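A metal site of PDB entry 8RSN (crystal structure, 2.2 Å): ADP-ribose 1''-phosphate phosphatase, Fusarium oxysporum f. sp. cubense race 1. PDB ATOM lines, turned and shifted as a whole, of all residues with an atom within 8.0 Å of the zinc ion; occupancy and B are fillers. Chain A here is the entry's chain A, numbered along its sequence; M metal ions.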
ATOM      1  N   GLN A 447      29.710   0.851 -17.892  1.00  0.00           N
ATOM      2  CA  GLN A 447      28.919  -0.155 -17.209  1.00  0.00           C
ATOM      3  C   GLN A 447      29.079  -1.524 -17.864  1.00  0.00           C
ATOM      4  O   GLN A 447      29.523  -1.648 -19.010  1.00  0.00           O
ATOM      5  CB  GLN A 447      27.416   0.202 -17.240  1.00  0.00           C
ATOM      6  CG  GLN A 447      26.757   0.097 -18.603  1.00  0.00           C
ATOM      7  CD  GLN A 447      25.232   0.037 -18.544  1.00  0.00           C
ATOM      8  OE1 GLN A 447      24.509   1.030 -18.731  1.00  0.00           O
ATOM      9  NE2 GLN A 447      24.695  -1.138 -18.302  1.00  0.00           N
ATOM     10  N   CYS A 448      28.605  -2.523 -17.111  1.00  0.00           N
ATOM     11  CA  CYS A 448      28.509  -3.895 -17.556  1.00  0.00           C
ATOM     12  C   CYS A 448      27.439  -4.030 -18.614  1.00  0.00           C
ATOM     13  O   CYS A 448      26.321  -3.613 -18.370  1.00  0.00           O
ATOM     14  CB  CYS A 448      28.146  -4.788 -16.371  1.00  0.00           C
ATOM     15  SG  CYS A 448      27.679  -6.483 -16.818  1.00  0.00           S
ATOM     16  N   LEU A 449      27.747  -4.716 -19.718  1.00  0.00           N
ATOM     17  CA  LEU A 449      26.895  -4.744 -20.897  1.00  0.00           C
ATOM     18  C   LEU A 449      25.767  -5.789 -20.771  1.00  0.00           C
ATOM     19  O   LEU A 449      24.760  -5.729 -21.493  1.00  0.00           O
ATOM     20  CB  LEU A 449      27.836  -4.997 -22.073  1.00  0.00           C
ATOM     21  CG  LEU A 449      27.319  -4.708 -23.487  1.00  0.00           C
ATOM     22  CD1 LEU A 449      26.568  -3.378 -23.610  1.00  0.00           C
ATOM     23  CD2 LEU A 449      28.518  -4.724 -24.440  1.00  0.00           C
ATOM     24  N   ASN A 450      25.898  -6.693 -19.790  1.00  0.00           N
ATOM     25  CA  ASN A 450      24.835  -7.597 -19.361  1.00  0.00           C
ATOM     26  C   ASN A 450      24.039  -7.018 -18.182  1.00  0.00           C
ATOM     27  O   ASN A 450      23.083  -7.644 -17.743  1.00  0.00           O
ATOM     28  CB  ASN A 450      25.384  -8.957 -18.907  1.00  0.00           C
ATOM     29  CG  ASN A 450      25.897  -9.782 -20.069  1.00  0.00           C
ATOM     30  OD1 ASN A 450      25.284  -9.748 -21.140  1.00  0.00           O
ATOM     31  ND2 ASN A 450      27.013 -10.471 -19.916  1.00  0.00           N
ATOM     32  N   ASN A 451      24.450  -5.849 -17.675  1.00  0.00           N
ATOM     33  CA  ASN A 451      23.767  -5.139 -16.609  1.00  0.00           C
ATOM     34  C   ASN A 451      23.450  -6.090 -15.461  1.00  0.00           C
ATOM     35  O   ASN A 451      22.301  -6.272 -15.084  1.00  0.00           O
ATOM     36  CB  ASN A 451      22.514  -4.441 -17.136  1.00  0.00           C
ATOM     37  CG  ASN A 451      21.919  -3.443 -16.170  1.00  0.00           C
ATOM     38  OD1 ASN A 451      22.615  -2.905 -15.296  1.00  0.00           O
ATOM     39  ND2 ASN A 451      20.644  -3.153 -16.356  1.00  0.00           N
ATOM     40  N   CYS A 452      24.467  -6.751 -14.937  1.00  0.00           N
ATOM     41  CA  CYS A 452      24.243  -7.869 -14.021  1.00  0.00           C
ATOM     42  C   CYS A 452      23.793  -7.402 -12.623  1.00  0.00           C
ATOM     43  O   CYS A 452      23.074  -8.145 -11.949  1.00  0.00           O
ATOM     44  CB  CYS A 452      25.493  -8.734 -13.934  1.00  0.00           C
ATOM     45  SG  CYS A 452      26.905  -7.909 -13.143  1.00  0.00           S
ATOM     46  N   ARG A 453      24.252  -6.206 -12.207  1.00  0.00           N
ATOM     47  CA  ARG A 453      23.803  -5.577 -10.967  1.00  0.00           C
ATOM     48  C   ARG A 453      23.895  -4.052 -11.095  1.00  0.00           C
ATOM     49  O   ARG A 453      24.627  -3.532 -11.926  1.00  0.00           O
ATOM     50  CB  ARG A 453      24.642  -6.047  -9.783  1.00  0.00           C
ATOM     51  CG  ARG A 453      25.821  -5.124  -9.495  1.00  0.00           C
ATOM     52  CD  ARG A 453      26.332  -5.145  -8.072  1.00  0.00           C
ATOM     53  NE  ARG A 453      26.861  -6.474  -7.763  1.00  0.00           N
ATOM     54  CZ  ARG A 453      27.450  -6.822  -6.610  1.00  0.00           C
ATOM     55  NH1 ARG A 453      28.123  -7.957  -6.552  1.00  0.00           N
ATOM     56  NH2 ARG A 453      27.407  -6.011  -5.561  1.00  0.00           N
ATOM     57  N   ASP A 455      25.326  -1.866  -9.208  1.00  0.00           N
ATOM     58  CA  ASP A 455      26.629  -1.312  -8.843  1.00  0.00           C
ATOM     59  C   ASP A 455      27.700  -1.522  -9.918  1.00  0.00           C
ATOM     60  O   ASP A 455      28.776  -0.942  -9.796  1.00  0.00           O
ATOM     61  CB  ASP A 455      27.198  -2.000  -7.579  1.00  0.00           C
ATOM     62  CG  ASP A 455      27.303  -1.101  -6.367  1.00  0.00           C
ATOM     63  OD1 ASP A 455      27.166   0.149  -6.556  1.00  0.00           O
ATOM     64  OD2 ASP A 455      27.555  -1.639  -5.243  1.00  0.00           O
ATOM     65  N   ALA A 456      27.420  -2.332 -10.952  1.00  0.00           N
ATOM     66  CA  ALA A 456      28.348  -2.613 -12.052  1.00  0.00           C
ATOM     67  C   ALA A 456      28.580  -1.405 -13.007  1.00  0.00           C
ATOM     68  O   ALA A 456      28.446  -1.584 -14.228  1.00  0.00           O
ATOM     69  CB  ALA A 456      27.825  -3.794 -12.841  1.00  0.00           C
ATOM     70  N   VAL A 457      29.047  -0.262 -12.459  1.00  0.00           N
ATOM     71  CA  VAL A 457      29.451   0.913 -13.220  1.00  0.00           C
ATOM     72  C   VAL A 457      30.783   1.399 -12.687  1.00  0.00           C
ATOM     73  O   VAL A 457      31.161   0.906 -11.647  1.00  0.00           O
ATOM     74  CB  VAL A 457      28.380   2.019 -13.124  1.00  0.00           C
ATOM     75  CG1 VAL A 457      27.006   1.478 -13.478  1.00  0.00           C
ATOM     76  CG2 VAL A 457      28.337   2.676 -11.747  1.00  0.00           C
ATOM     77  N   LEU A 486      36.581  -4.783 -17.990  1.00  0.00           N
ATOM     78  CA  LEU A 486      35.649  -5.902 -17.871  1.00  0.00           C
ATOM     79  C   LEU A 486      34.853  -5.725 -16.571  1.00  0.00           C
ATOM     80  O   LEU A 486      35.368  -5.087 -15.641  1.00  0.00           O
ATOM     81  CB  LEU A 486      36.451  -7.209 -17.852  1.00  0.00           C
ATOM     82  CG  LEU A 486      37.146  -7.586 -19.162  1.00  0.00           C
ATOM     83  CD1 LEU A 486      37.984  -8.858 -18.973  1.00  0.00           C
ATOM     84  CD2 LEU A 486      36.141  -7.784 -20.296  1.00  0.00           C
ATOM     85  N   CYS A 487      33.582  -6.201 -16.553  1.00  0.00           N
ATOM     86  CA  CYS A 487      32.771  -6.134 -15.330  1.00  0.00           C
ATOM     87  C   CYS A 487      33.523  -6.881 -14.226  1.00  0.00           C
ATOM     88  O   CYS A 487      33.693  -8.135 -14.310  1.00  0.00           O
ATOM     89  CB  CYS A 487      31.375  -6.761 -15.419  1.00  0.00           C
ATOM     90  SG  CYS A 487      30.295  -6.618 -13.940  1.00  0.00           S
ATOM     91  N   ARG A 488      33.921  -6.100 -13.204  1.00  0.00           N
ATOM     92  CA  ARG A 488      34.668  -6.567 -12.049  1.00  0.00           C
ATOM     93  C   ARG A 488      33.898  -7.631 -11.239  1.00  0.00           C
ATOM     94  O   ARG A 488      34.466  -8.144 -10.278  1.00  0.00           O
ATOM     95  CB  ARG A 488      35.041  -5.347 -11.206  1.00  0.00           C
ATOM     96  CG  ARG A 488      33.977  -4.898 -10.209  1.00  0.00           C
ATOM     97  CD  ARG A 488      34.292  -3.545  -9.622  1.00  0.00           C
ATOM     98  NE  ARG A 488      33.147  -3.038  -8.855  1.00  0.00           N
ATOM     99  CZ  ARG A 488      32.233  -2.158  -9.276  1.00  0.00           C
ATOM    100  NH1 ARG A 488      32.189  -1.733 -10.536  1.00  0.00           N
ATOM    101  NH2 ARG A 488      31.315  -1.729  -8.427  1.00  0.00           N
ATOM    102  N   PHE A 489      32.671  -8.013 -11.644  1.00  0.00           N
ATOM    103  CA  PHE A 489      31.814  -8.936 -10.920  1.00  0.00           C
ATOM    104  C   PHE A 489      31.473 -10.131 -11.821  1.00  0.00           C
ATOM    105  O   PHE A 489      31.606 -11.271 -11.367  1.00  0.00           O
ATOM    106  CB  PHE A 489      30.473  -8.346 -10.445  1.00  0.00           C
ATOM    107  CG  PHE A 489      30.550  -7.128  -9.543  1.00  0.00           C
ATOM    108  CD1 PHE A 489      31.340  -7.120  -8.396  1.00  0.00           C
ATOM    109  CD2 PHE A 489      29.815  -5.990  -9.829  1.00  0.00           C
ATOM    110  CE1 PHE A 489      31.407  -5.991  -7.581  1.00  0.00           C
ATOM    111  CE2 PHE A 489      29.883  -4.866  -9.005  1.00  0.00           C
ATOM    112  CZ  PHE A 489      30.679  -4.869  -7.877  1.00  0.00           C
ATOM    113  N   CYS A 490      30.946  -9.906 -13.038  1.00  0.00           N
ATOM    114  CA  CYS A 490      30.656 -11.037 -13.925  1.00  0.00           C
ATOM    115  C   CYS A 490      31.738 -11.219 -14.996  1.00  0.00           C
ATOM    116  O   CYS A 490      31.689 -12.186 -15.737  1.00  0.00           O
ATOM    117  CB  CYS A 490      29.239 -10.962 -14.514  1.00  0.00           C
ATOM    118  SG  CYS A 490      28.937  -9.718 -15.819  1.00  0.00           S
ATOM    119  N   GLY A 491      32.694 -10.278 -15.095  1.00  0.00           N
ATOM    120  CA  GLY A 491      33.717 -10.270 -16.130  1.00  0.00           C
ATOM    121  C   GLY A 491      33.210 -10.062 -17.569  1.00  0.00           C
ATOM    122  O   GLY A 491      33.935 -10.280 -18.528  1.00  0.00           O
ATOM    123  N   SER A 492      31.980  -9.585 -17.762  1.00  0.00           N
ATOM    124  CA  SER A 492      31.535  -9.407 -19.128  1.00  0.00           C
ATOM    125  C   SER A 492      32.104  -8.088 -19.682  1.00  0.00           C
ATOM    126  O   SER A 492      32.690  -7.246 -18.971  1.00  0.00           O
ATOM    127  CB  SER A 492      30.034  -9.513 -19.261  1.00  0.00           C
ATOM    128  OG  SER A 492      29.416  -8.232 -19.374  1.00  0.00           O
ATOM    129  N   LYS A 493      31.965  -7.983 -21.001  1.00  0.00           N
ATOM    130  CA  LYS A 493      32.282  -6.765 -21.709  1.00  0.00           C
ATOM    131  C   LYS A 493      31.573  -5.552 -21.088  1.00  0.00           C
ATOM    132  O   LYS A 493      30.505  -5.639 -20.483  1.00  0.00           O
ATOM    133  CB  LYS A 493      31.859  -6.920 -23.172  1.00  0.00           C
ATOM    134  CG  LYS A 493      32.598  -7.978 -23.981  1.00  0.00           C
ATOM    135  CD  LYS A 493      31.995  -8.177 -25.357  1.00  0.00           C
ATOM    136  CE  LYS A 493      32.673  -9.313 -26.082  1.00  0.00           C
ATOM    137  NZ  LYS A 493      34.144  -9.098 -26.127  1.00  0.00           N
ATOM    138  N   MET A 494      32.151  -4.373 -21.329  1.00  0.00           N
ATOM    139  CA  MET A 494      31.561  -3.138 -20.841  1.00  0.00           C
ATOM    140  C   MET A 494      31.285  -2.171 -21.986  1.00  0.00           C
ATOM    141  O   MET A 494      31.620  -2.442 -23.134  1.00  0.00           O
ATOM    142  CB  MET A 494      32.486  -2.569 -19.795  1.00  0.00           C
ATOM    143  CG  MET A 494      32.302  -3.396 -18.532  1.00  0.00           C
ATOM    144  SD  MET A 494      33.281  -2.519 -17.339  1.00  0.00           S
ATOM    145  CE  MET A 494      32.072  -1.907 -16.180  1.00  0.00           C
HETATM  146 ZN    ZN M   1      28.478  -7.627 -14.881  1.00  0.00          ZN
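N of Cys 448 sits at hydrogen-bond distance from O of Ala 456 (3.0 Å).
N of Phe 489 sits close to SG of Cys 487, at 3.6 Å.
N of Cys 487 sits close to SD of Met 494, 3.8 Å away.
N of Cys 487 lies within hydrogen-bond range of O of Ser 492 (2.8 Å).
The side-chain sulfur (SG) of Cys 490 lies close to the backbone NH (N) of Ser 492 (3.6 Å).
The side-chain sulfur of Cys 448 sits close to the backbone NH of Asn 450 (3.5 Å).
The side-chain sulfur of Cys 448 sits close to the side-chain hydroxyl of Ser 492 (3.6 Å).
The side-chain sulfur of Cys 448 sits close to the backbone NH of Asn 451, 3.4 Å away.
The zinc ion is bound by SG of Cys 487 (2.3 Å), SG of Cys 490 (2.3 Å), SG of Cys 452 (2.4 Å) and SG of Cys 448 (2.4 Å).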
